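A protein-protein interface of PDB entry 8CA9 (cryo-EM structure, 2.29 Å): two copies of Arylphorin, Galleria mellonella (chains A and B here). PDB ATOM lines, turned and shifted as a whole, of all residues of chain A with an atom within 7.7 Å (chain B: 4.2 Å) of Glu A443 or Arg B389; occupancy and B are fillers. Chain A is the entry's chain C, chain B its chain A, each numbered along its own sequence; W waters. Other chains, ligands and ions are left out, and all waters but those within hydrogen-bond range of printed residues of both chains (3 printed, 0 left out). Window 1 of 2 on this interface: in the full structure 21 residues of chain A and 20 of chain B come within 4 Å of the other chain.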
ATOM      1  N   PHE A 341     -20.915  -0.719   3.725  1.00  0.00           N
ATOM      2  CA  PHE A 341     -19.485  -0.442   3.732  1.00  0.00           C
ATOM      3  C   PHE A 341     -19.008  -0.114   5.138  1.00  0.00           C
ATOM      4  O   PHE A 341     -17.990  -0.646   5.597  1.00  0.00           O
ATOM      5  CB  PHE A 341     -19.163   0.703   2.772  1.00  0.00           C
ATOM      6  CG  PHE A 341     -17.692   0.898   2.537  1.00  0.00           C
ATOM      7  CD1 PHE A 341     -16.991   0.033   1.715  1.00  0.00           C
ATOM      8  CD2 PHE A 341     -17.010   1.944   3.136  1.00  0.00           C
ATOM      9  CE1 PHE A 341     -15.639   0.206   1.496  1.00  0.00           C
ATOM     10  CE2 PHE A 341     -15.658   2.122   2.919  1.00  0.00           C
ATOM     11  CZ  PHE A 341     -14.971   1.252   2.098  1.00  0.00           C
ATOM     12  N   LEU A 342     -19.758   0.726   5.857  1.00  0.00           N
ATOM     13  CA  LEU A 342     -19.354   1.072   7.213  1.00  0.00           C
ATOM     14  C   LEU A 342     -19.256  -0.177   8.076  1.00  0.00           C
ATOM     15  O   LEU A 342     -18.288  -0.349   8.828  1.00  0.00           O
ATOM     16  CB  LEU A 342     -20.336   2.075   7.817  1.00  0.00           C
ATOM     17  CG  LEU A 342     -20.379   3.454   7.155  1.00  0.00           C
ATOM     18  CD1 LEU A 342     -21.443   4.328   7.800  1.00  0.00           C
ATOM     19  CD2 LEU A 342     -19.019   4.131   7.222  1.00  0.00           C
ATOM     20  N   LEU A 345     -16.057  -1.806   7.582  1.00  0.00           N
ATOM     21  CA  LEU A 345     -14.961  -1.142   8.276  1.00  0.00           C
ATOM     22  C   LEU A 345     -14.876  -1.588   9.729  1.00  0.00           C
ATOM     23  O   LEU A 345     -13.784  -1.598  10.312  1.00  0.00           O
ATOM     24  CB  LEU A 345     -15.122   0.376   8.193  1.00  0.00           C
ATOM     25  CG  LEU A 345     -15.102   0.979   6.786  1.00  0.00           C
ATOM     26  CD1 LEU A 345     -15.189   2.494   6.854  1.00  0.00           C
ATOM     27  CD2 LEU A 345     -13.857   0.550   6.025  1.00  0.00           C
ATOM     28  N   GLN A 346     -16.006  -1.960  10.331  1.00  0.00           N
ATOM     29  CA  GLN A 346     -15.974  -2.477  11.694  1.00  0.00           C
ATOM     30  C   GLN A 346     -15.476  -3.915  11.742  1.00  0.00           C
ATOM     31  O   GLN A 346     -14.866  -4.321  12.737  1.00  0.00           O
ATOM     32  CB  GLN A 346     -17.363  -2.379  12.326  1.00  0.00           C
ATOM     33  CG  GLN A 346     -17.802  -0.958  12.634  1.00  0.00           C
ATOM     34  CD  GLN A 346     -16.983  -0.323  13.740  1.00  0.00           C
ATOM     35  OE1 GLN A 346     -16.609  -0.984  14.709  1.00  0.00           O
ATOM     36  NE2 GLN A 346     -16.696   0.966  13.599  1.00  0.00           N
ATOM     37  N   ILE A 437     -18.004   9.577  -2.123  1.00  0.00           N
ATOM     38  CA  ILE A 437     -17.427   8.247  -2.326  1.00  0.00           C
ATOM     39  C   ILE A 437     -15.965   8.226  -1.886  1.00  0.00           C
ATOM     40  O   ILE A 437     -15.515   7.294  -1.207  1.00  0.00           O
ATOM     41  CB  ILE A 437     -17.587   7.812  -3.795  1.00  0.00           C
ATOM     42  CG1 ILE A 437     -19.072   7.665  -4.140  1.00  0.00           C
ATOM     43  CG2 ILE A 437     -16.842   6.503  -4.041  1.00  0.00           C
ATOM     44  CD1 ILE A 437     -19.349   7.426  -5.610  1.00  0.00           C
ATOM     45  N   LEU A 438     -15.198   9.251  -2.266  1.00  0.00           N
ATOM     46  CA  LEU A 438     -13.795   9.304  -1.873  1.00  0.00           C
ATOM     47  C   LEU A 438     -13.636   9.515  -0.375  1.00  0.00           C
ATOM     48  O   LEU A 438     -12.641   9.071   0.202  1.00  0.00           O
ATOM     49  CB  LEU A 438     -13.064  10.407  -2.639  1.00  0.00           C
ATOM     50  CG  LEU A 438     -12.924  10.255  -4.157  1.00  0.00           C
ATOM     51  CD1 LEU A 438     -11.756  11.087  -4.645  1.00  0.00           C
ATOM     52  CD2 LEU A 438     -12.757   8.803  -4.578  1.00  0.00           C
ATOM     53  N   ASP A 439     -14.581  10.196   0.274  1.00  0.00           N
ATOM     54  CA  ASP A 439     -14.538  10.298   1.729  1.00  0.00           C
ATOM     55  C   ASP A 439     -14.683   8.925   2.369  1.00  0.00           C
ATOM     56  O   ASP A 439     -13.958   8.589   3.313  1.00  0.00           O
ATOM     57  CB  ASP A 439     -15.631  11.241   2.229  1.00  0.00           C
ATOM     58  CG  ASP A 439     -15.348  12.693   1.898  1.00  0.00           C
ATOM     59  OD1 ASP A 439     -14.157  13.068   1.831  1.00  0.00           O
ATOM     60  OD2 ASP A 439     -16.314  13.460   1.709  1.00  0.00           O
ATOM     61  N   TYR A 440     -15.613   8.111   1.863  1.00  0.00           N
ATOM     62  CA  TYR A 440     -15.710   6.736   2.355  1.00  0.00           C
ATOM     63  C   TYR A 440     -14.408   5.978   2.111  1.00  0.00           C
ATOM     64  O   TYR A 440     -13.914   5.255   2.989  1.00  0.00           O
ATOM     65  CB  TYR A 440     -16.878   6.007   1.690  1.00  0.00           C
ATOM     66  CG  TYR A 440     -18.243   6.404   2.202  1.00  0.00           C
ATOM     67  CD1 TYR A 440     -18.624   6.135   3.511  1.00  0.00           C
ATOM     68  CD2 TYR A 440     -19.161   7.027   1.369  1.00  0.00           C
ATOM     69  CE1 TYR A 440     -19.876   6.492   3.977  1.00  0.00           C
ATOM     70  CE2 TYR A 440     -20.412   7.386   1.826  1.00  0.00           C
ATOM     71  CZ  TYR A 440     -20.766   7.116   3.128  1.00  0.00           C
ATOM     72  OH  TYR A 440     -22.014   7.474   3.581  1.00  0.00           O
ATOM     73  N   ILE A 441     -13.835   6.131   0.915  1.00  0.00           N
ATOM     74  CA  ILE A 441     -12.618   5.386   0.600  1.00  0.00           C
ATOM     75  C   ILE A 441     -11.458   5.836   1.484  1.00  0.00           C
ATOM     76  O   ILE A 441     -10.621   5.019   1.874  1.00  0.00           O
ATOM     77  CB  ILE A 441     -12.274   5.510  -0.896  1.00  0.00           C
ATOM     78  CG1 ILE A 441     -13.349   4.816  -1.740  1.00  0.00           C
ATOM     79  CG2 ILE A 441     -10.908   4.894  -1.169  1.00  0.00           C
ATOM     80  CD1 ILE A 441     -13.205   5.025  -3.236  1.00  0.00           C
ATOM     81  N   ASN A 442     -11.384   7.125   1.825  1.00  0.00           N
ATOM     82  CA  ASN A 442     -10.327   7.595   2.717  1.00  0.00           C
ATOM     83  C   ASN A 442     -10.560   7.120   4.146  1.00  0.00           C
ATOM     84  O   ASN A 442      -9.602   6.827   4.876  1.00  0.00           O
ATOM     85  CB  ASN A 442     -10.235   9.119   2.673  1.00  0.00           C
ATOM     86  CG  ASN A 442      -9.870   9.643   1.299  1.00  0.00           C
ATOM     87  OD1 ASN A 442      -9.077   9.036   0.580  1.00  0.00           O
ATOM     88  ND2 ASN A 442     -10.452  10.776   0.928  1.00  0.00           N
ATOM     89  N   GLU A 443     -11.823   7.053   4.571  1.00  0.00           N
ATOM     90  CA  GLU A 443     -12.116   6.441   5.860  1.00  0.00           C
ATOM     91  C   GLU A 443     -11.589   5.014   5.892  1.00  0.00           C
ATOM     92  O   GLU A 443     -11.029   4.569   6.900  1.00  0.00           O
ATOM     93  CB  GLU A 443     -13.622   6.477   6.133  1.00  0.00           C
ATOM     94  CG  GLU A 443     -13.977   6.393   7.610  1.00  0.00           C
ATOM     95  CD  GLU A 443     -13.568   7.636   8.381  1.00  0.00           C
ATOM     96  OE1 GLU A 443     -13.056   8.587   7.751  1.00  0.00           O
ATOM     97  OE2 GLU A 443     -13.757   7.664   9.615  1.00  0.00           O
ATOM     98  N   TYR A 444     -11.749   4.286   4.783  1.00  0.00           N
ATOM     99  CA  TYR A 444     -11.125   2.969   4.673  1.00  0.00           C
ATOM    100  C   TYR A 444      -9.604   3.066   4.735  1.00  0.00           C
ATOM    101  O   TYR A 444      -8.951   2.279   5.430  1.00  0.00           O
ATOM    102  CB  TYR A 444     -11.540   2.294   3.369  1.00  0.00           C
ATOM    103  CG  TYR A 444     -10.416   1.496   2.745  1.00  0.00           C
ATOM    104  CD1 TYR A 444     -10.020   0.279   3.280  1.00  0.00           C
ATOM    105  CD2 TYR A 444      -9.741   1.970   1.628  1.00  0.00           C
ATOM    106  CE1 TYR A 444      -8.989  -0.445   2.717  1.00  0.00           C
ATOM    107  CE2 TYR A 444      -8.712   1.251   1.058  1.00  0.00           C
ATOM    108  CZ  TYR A 444      -8.340   0.044   1.607  1.00  0.00           C
ATOM    109  OH  TYR A 444      -7.312  -0.669   1.035  1.00  0.00           O
ATOM    110  N   LYS A 445      -9.027   4.015   3.998  1.00  0.00           N
ATOM    111  CA  LYS A 445      -7.579   4.168   3.930  1.00  0.00           C
ATOM    112  C   LYS A 445      -6.962   4.385   5.298  1.00  0.00           C
ATOM    113  O   LYS A 445      -5.806   4.006   5.513  1.00  0.00           O
ATOM    114  CB  LYS A 445      -7.217   5.353   3.036  1.00  0.00           C
ATOM    115  CG  LYS A 445      -7.451   5.162   1.551  1.00  0.00           C
ATOM    116  CD  LYS A 445      -6.325   4.383   0.887  1.00  0.00           C
ATOM    117  CE  LYS A 445      -6.466   4.398  -0.629  1.00  0.00           C
ATOM    118  NZ  LYS A 445      -5.382   3.639  -1.312  1.00  0.00           N
ATOM    119  N   GLU A 446      -7.701   5.008   6.215  1.00  0.00           N
ATOM    120  CA  GLU A 446      -7.174   5.244   7.556  1.00  0.00           C
ATOM    121  C   GLU A 446      -6.648   3.969   8.209  1.00  0.00           C
ATOM    122  O   GLU A 446      -5.878   4.059   9.171  1.00  0.00           O
ATOM    123  CB  GLU A 446      -8.250   5.862   8.450  1.00  0.00           C
ATOM    124  CG  GLU A 446      -8.689   7.255   8.036  1.00  0.00           C
ATOM    125  CD  GLU A 446      -9.574   7.922   9.076  1.00  0.00           C
ATOM    126  OE1 GLU A 446      -9.496   7.539  10.263  1.00  0.00           O
ATOM    127  OE2 GLU A 446     -10.349   8.828   8.702  1.00  0.00           O
ATOM    128  N   TYR A 447      -7.047   2.793   7.718  1.00  0.00           N
ATOM    129  CA  TYR A 447      -6.542   1.538   8.268  1.00  0.00           C
ATOM    130  C   TYR A 447      -5.045   1.373   8.039  1.00  0.00           C
ATOM    131  O   TYR A 447      -4.339   0.867   8.921  1.00  0.00           O
ATOM    132  CB  TYR A 447      -7.283   0.356   7.638  1.00  0.00           C
ATOM    133  CG  TYR A 447      -8.361  -0.252   8.503  1.00  0.00           C
ATOM    134  CD1 TYR A 447      -9.652   0.260   8.504  1.00  0.00           C
ATOM    135  CD2 TYR A 447      -8.092  -1.351   9.306  1.00  0.00           C
ATOM    136  CE1 TYR A 447     -10.640  -0.301   9.290  1.00  0.00           C
ATOM    137  CE2 TYR A 447      -9.072  -1.918  10.092  1.00  0.00           C
ATOM    138  CZ  TYR A 447     -10.344  -1.391  10.082  1.00  0.00           C
ATOM    139  OH  TYR A 447     -11.323  -1.954  10.866  1.00  0.00           O
ATOM    140  N   LEU A 448      -4.546   1.779   6.876  1.00  0.00           N
ATOM    141  CA  LEU A 448      -3.189   1.434   6.473  1.00  0.00           C
ATOM    142  C   LEU A 448      -2.155   2.077   7.390  1.00  0.00           C
ATOM    143  O   LEU A 448      -2.337   3.189   7.894  1.00  0.00           O
ATOM    144  CB  LEU A 448      -2.938   1.868   5.030  1.00  0.00           C
ATOM    145  CG  LEU A 448      -3.970   1.401   4.001  1.00  0.00           C
ATOM    146  CD1 LEU A 448      -3.594   1.884   2.610  1.00  0.00           C
ATOM    147  CD2 LEU A 448      -4.118  -0.113   4.023  1.00  0.00           C
ATOM    148  N   TRP A 549      -2.559  15.903   1.880  1.00  0.00           N
ATOM    149  CA  TRP A 549      -2.029  14.785   1.104  1.00  0.00           C
ATOM    150  C   TRP A 549      -2.986  14.361  -0.004  1.00  0.00           C
ATOM    151  O   TRP A 549      -2.540  13.916  -1.068  1.00  0.00           O
ATOM    152  CB  TRP A 549      -1.717  13.602   2.022  1.00  0.00           C
ATOM    153  CG  TRP A 549      -2.913  13.026   2.710  1.00  0.00           C
ATOM    154  CD1 TRP A 549      -3.516  13.500   3.834  1.00  0.00           C
ATOM    155  CD2 TRP A 549      -3.647  11.859   2.322  1.00  0.00           C
ATOM    156  NE1 TRP A 549      -4.583  12.704   4.172  1.00  0.00           N
ATOM    157  CE2 TRP A 549      -4.685  11.689   3.259  1.00  0.00           C
ATOM    158  CE3 TRP A 549      -3.529  10.943   1.272  1.00  0.00           C
ATOM    159  CZ2 TRP A 549      -5.599  10.642   3.177  1.00  0.00           C
ATOM    160  CZ3 TRP A 549      -4.437   9.904   1.195  1.00  0.00           C
ATOM    161  CH2 TRP A 549      -5.458   9.761   2.141  1.00  0.00           C
ATOM    162  N   PRO A 661      -2.776   7.922   4.124  1.00  0.00           N
ATOM    163  CA  PRO A 661      -2.798   9.115   4.978  1.00  0.00           C
ATOM    164  C   PRO A 661      -1.451   9.393   5.626  1.00  0.00           C
ATOM    165  O   PRO A 661      -0.694   8.481   5.969  1.00  0.00           O
ATOM    166  CB  PRO A 661      -3.856   8.780   6.036  1.00  0.00           C
ATOM    167  CG  PRO A 661      -4.675   7.693   5.443  1.00  0.00           C
ATOM    168  CD  PRO A 661      -3.759   6.916   4.557  1.00  0.00           C
ATOM    169  N   ASP B 330     -20.845  11.830  10.320  1.00  0.00           N
ATOM    170  CA  ASP B 330     -21.026  11.383  11.695  1.00  0.00           C
ATOM    171  C   ASP B 330     -22.400  10.759  11.877  1.00  0.00           C
ATOM    172  O   ASP B 330     -22.523   9.623  12.353  1.00  0.00           O
ATOM    173  CB  ASP B 330     -20.835  12.559  12.656  1.00  0.00           C
ATOM    174  CG  ASP B 330     -19.383  12.978  12.786  1.00  0.00           C
ATOM    175  OD1 ASP B 330     -18.517  12.340  12.150  1.00  0.00           O
ATOM    176  OD2 ASP B 330     -19.108  13.946  13.525  1.00  0.00           O
ATOM    177  N   PHE B 333     -22.614   7.220  10.624  1.00  0.00           N
ATOM    178  CA  PHE B 333     -21.962   6.275  11.518  1.00  0.00           C
ATOM    179  C   PHE B 333     -22.871   5.958  12.693  1.00  0.00           C
ATOM    180  O   PHE B 333     -23.201   4.791  12.943  1.00  0.00           O
ATOM    181  CB  PHE B 333     -20.624   6.844  11.998  1.00  0.00           C
ATOM    182  CG  PHE B 333     -19.949   6.009  13.049  1.00  0.00           C
ATOM    183  CD1 PHE B 333     -19.135   4.946  12.696  1.00  0.00           C
ATOM    184  CD2 PHE B 333     -20.120   6.296  14.392  1.00  0.00           C
ATOM    185  CE1 PHE B 333     -18.513   4.181  13.664  1.00  0.00           C
ATOM    186  CE2 PHE B 333     -19.501   5.534  15.363  1.00  0.00           C
ATOM    187  CZ  PHE B 333     -18.696   4.476  14.999  1.00  0.00           C
ATOM    188  N   SER B 374     -17.579   1.408  23.281  1.00  0.00           N
ATOM    189  CA  SER B 374     -16.476   1.413  22.321  1.00  0.00           C
ATOM    190  C   SER B 374     -15.129   1.449  23.037  1.00  0.00           C
ATOM    191  O   SER B 374     -14.186   2.106  22.591  1.00  0.00           O
ATOM    192  CB  SER B 374     -16.600   2.587  21.346  1.00  0.00           C
ATOM    193  OG  SER B 374     -17.840   2.554  20.664  1.00  0.00           O
ATOM    194  N   TYR B 379     -12.125  -4.461  21.426  1.00  0.00           N
ATOM    195  CA  TYR B 379     -11.213  -4.770  20.329  1.00  0.00           C
ATOM    196  C   TYR B 379      -9.969  -5.506  20.818  1.00  0.00           C
ATOM    197  O   TYR B 379      -8.881  -5.348  20.263  1.00  0.00           O
ATOM    198  CB  TYR B 379     -10.805  -3.495  19.595  1.00  0.00           C
ATOM    199  CG  TYR B 379     -11.942  -2.537  19.320  1.00  0.00           C
ATOM    200  CD1 TYR B 379     -12.756  -2.693  18.208  1.00  0.00           C
ATOM    201  CD2 TYR B 379     -12.191  -1.467  20.169  1.00  0.00           C
ATOM    202  CE1 TYR B 379     -13.792  -1.815  17.952  1.00  0.00           C
ATOM    203  CE2 TYR B 379     -13.224  -0.584  19.922  1.00  0.00           C
ATOM    204  CZ  TYR B 379     -14.021  -0.764  18.811  1.00  0.00           C
ATOM    205  OH  TYR B 379     -15.051   0.113  18.562  1.00  0.00           O
ATOM    206  N   TYR B 387      -7.666   2.564  12.673  1.00  0.00           N
ATOM    207  CA  TYR B 387      -8.989   3.141  12.488  1.00  0.00           C
ATOM    208  C   TYR B 387      -9.844   2.836  13.710  1.00  0.00           C
ATOM    209  O   TYR B 387      -9.996   1.671  14.093  1.00  0.00           O
ATOM    210  CB  TYR B 387      -9.646   2.586  11.222  1.00  0.00           C
ATOM    211  CG  TYR B 387     -11.139   2.816  11.141  1.00  0.00           C
ATOM    212  CD1 TYR B 387     -11.653   3.997  10.625  1.00  0.00           C
ATOM    213  CD2 TYR B 387     -12.034   1.846  11.573  1.00  0.00           C
ATOM    214  CE1 TYR B 387     -13.017   4.209  10.548  1.00  0.00           C
ATOM    215  CE2 TYR B 387     -13.399   2.048  11.500  1.00  0.00           C
ATOM    216  CZ  TYR B 387     -13.884   3.231  10.986  1.00  0.00           C
ATOM    217  OH  TYR B 387     -15.242   3.436  10.911  1.00  0.00           O
ATOM    218  N   TRP B 388     -10.398   3.883  14.316  1.00  0.00           N
ATOM    219  CA  TRP B 388     -11.207   3.739  15.518  1.00  0.00           C
ATOM    220  C   TRP B 388     -12.201   4.887  15.587  1.00  0.00           C
ATOM    221  O   TRP B 388     -11.857   6.032  15.284  1.00  0.00           O
ATOM    222  CB  TRP B 388     -10.333   3.718  16.778  1.00  0.00           C
ATOM    223  CG  TRP B 388     -11.116   3.780  18.055  1.00  0.00           C
ATOM    224  CD1 TRP B 388     -11.760   2.748  18.671  1.00  0.00           C
ATOM    225  CD2 TRP B 388     -11.335   4.936  18.876  1.00  0.00           C
ATOM    226  NE1 TRP B 388     -12.368   3.188  19.822  1.00  0.00           N
ATOM    227  CE2 TRP B 388     -12.122   4.527  19.971  1.00  0.00           C
ATOM    228  CE3 TRP B 388     -10.942   6.275  18.789  1.00  0.00           C
ATOM    229  CZ2 TRP B 388     -12.523   5.409  20.972  1.00  0.00           C
ATOM    230  CZ3 TRP B 388     -11.343   7.150  19.785  1.00  0.00           C
ATOM    231  CH2 TRP B 388     -12.124   6.712  20.861  1.00  0.00           C
ATOM    232  N   ARG B 389     -13.432   4.571  15.984  1.00  0.00           N
ATOM    233  CA  ARG B 389     -14.467   5.574  16.175  1.00  0.00           C
ATOM    234  C   ARG B 389     -15.375   5.149  17.316  1.00  0.00           C
ATOM    235  O   ARG B 389     -15.651   3.959  17.492  1.00  0.00           O
ATOM    236  CB  ARG B 389     -15.293   5.785  14.903  1.00  0.00           C
ATOM    237  CG  ARG B 389     -14.494   6.298  13.721  1.00  0.00           C
ATOM    238  CD  ARG B 389     -15.422   6.718  12.600  1.00  0.00           C
ATOM    239  NE  ARG B 389     -16.266   7.832  13.013  1.00  0.00           N
ATOM    240  CZ  ARG B 389     -17.103   8.486  12.218  1.00  0.00           C
ATOM    241  NH1 ARG B 389     -17.232   8.172  10.940  1.00  0.00           N
ATOM    242  NH2 ARG B 389     -17.826   9.482  12.721  1.00  0.00           N
ATOM    243  N   SER B 390     -15.839   6.130  18.084  1.00  0.00           N
ATOM    244  CA  SER B 390     -16.660   5.897  19.264  1.00  0.00           C
ATOM    245  C   SER B 390     -18.057   6.459  19.041  1.00  0.00           C
ATOM    246  O   SER B 390     -18.210   7.606  18.609  1.00  0.00           O
ATOM    247  CB  SER B 390     -16.026   6.539  20.499  1.00  0.00           C
ATOM    248  OG  SER B 390     -16.878   6.432  21.625  1.00  0.00           O
ATOM    249  N   THR B 394     -18.952  10.546  19.045  1.00  0.00           N
ATOM    250  CA  THR B 394     -19.629  11.146  17.900  1.00  0.00           C
ATOM    251  C   THR B 394     -20.954  11.775  18.314  1.00  0.00           C
ATOM    252  O   THR B 394     -21.292  12.881  17.873  1.00  0.00           O
ATOM    253  CB  THR B 394     -19.850  10.093  16.814  1.00  0.00           C
ATOM    254  OG1 THR B 394     -18.620   9.403  16.556  1.00  0.00           O
ATOM    255  CG2 THR B 394     -20.334  10.739  15.528  1.00  0.00           C
HETATM  256  O   HOH W   1     -16.177   5.494   9.728  1.00  0.00           O
HETATM  257  O   HOH W   2     -14.086   1.198  15.653  1.00  0.00           O
HETATM  258  O   HOH W   3     -18.116   2.343  10.774  1.00  0.00           O
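The guanidinium group (NH1) of Arg B389 is in salt-bridge range of the side-chain carboxylate (OE2) of Glu A443, at 3.8 Å.
Of the 18 printed residues of chain A, 4 touch a printed residue of chain B.
Hydrophobic or aromatic side chains of chain A that line the printed part of chain B: Tyr A447.
Hydrophobic or aromatic side chains of chain B that line the printed part of chain A: Phe B333 and Tyr B387.
Among the printed residues, 6 pairs touch across the chains.
Among the printed residues, Asp or Glu carboxylates within 4 Å of a Lys or Arg side-chain nitrogen of the other chain: Glu A443 with Arg B389 (3.8 Å).
The guanidinium group (NH2) of Arg B389 is in salt-bridge range of the side-chain carboxylate (OD1) of Asp B330, at 3.0 Å.
O of Leu A345 is in hydrogen-bond range of OH of Tyr A447 (2.5 Å).
Of the printed residues of chain B, Leu A345 touches Tyr B387.
Leu A438 touches none of the printed residues of chain B.
Glu A443 touches just these residues of chain B: Tyr B387 (3.7 Å) and Arg B389 (3.5 Å).
Of the printed residues of chain B, Tyr A447 touches Tyr B387.
The nearest residue of chain A that does not touch Arg B389 is Gln A346 (5.0 Å).
The nearest printed residue of chain A that does not touch Tyr B387 is Glu A446 (4.2 Å).
Water W1 lies within hydrogen-bond range of OH of Tyr B387 (2.6 Å), NH1 of Arg B389 (3.1 Å) and OE2 of Glu A443 (3.3 Å).
Water W3 lies within hydrogen-bond range of the side-chain hydroxyl of Tyr B387 (3.1 Å), the backbone carbonyl oxygen of Leu A342 (3.3 Å) and the side-chain amide nitrogen of Gln A346 (3.4 Å).
Water W2 lies within hydrogen-bond range of OH of Tyr B379 (3.3 Å), NE2 of Gln A346 (3.3 Å) and N of Arg B389 (3.5 Å).
Tyr B387 touches Leu A345 (CE2 to O, 3.9 Å).
Gln A346 touches Phe B333.
Gln A346 touches Tyr B387 (NE2 to OH, 3.9 Å).
Tyr B387 touches Glu A443 (CE1 to OE2, 3.7 Å).
CE1 of Tyr A447 touches CD2 of Tyr B387, 3.4 Å away.
No position is printed for both chains.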
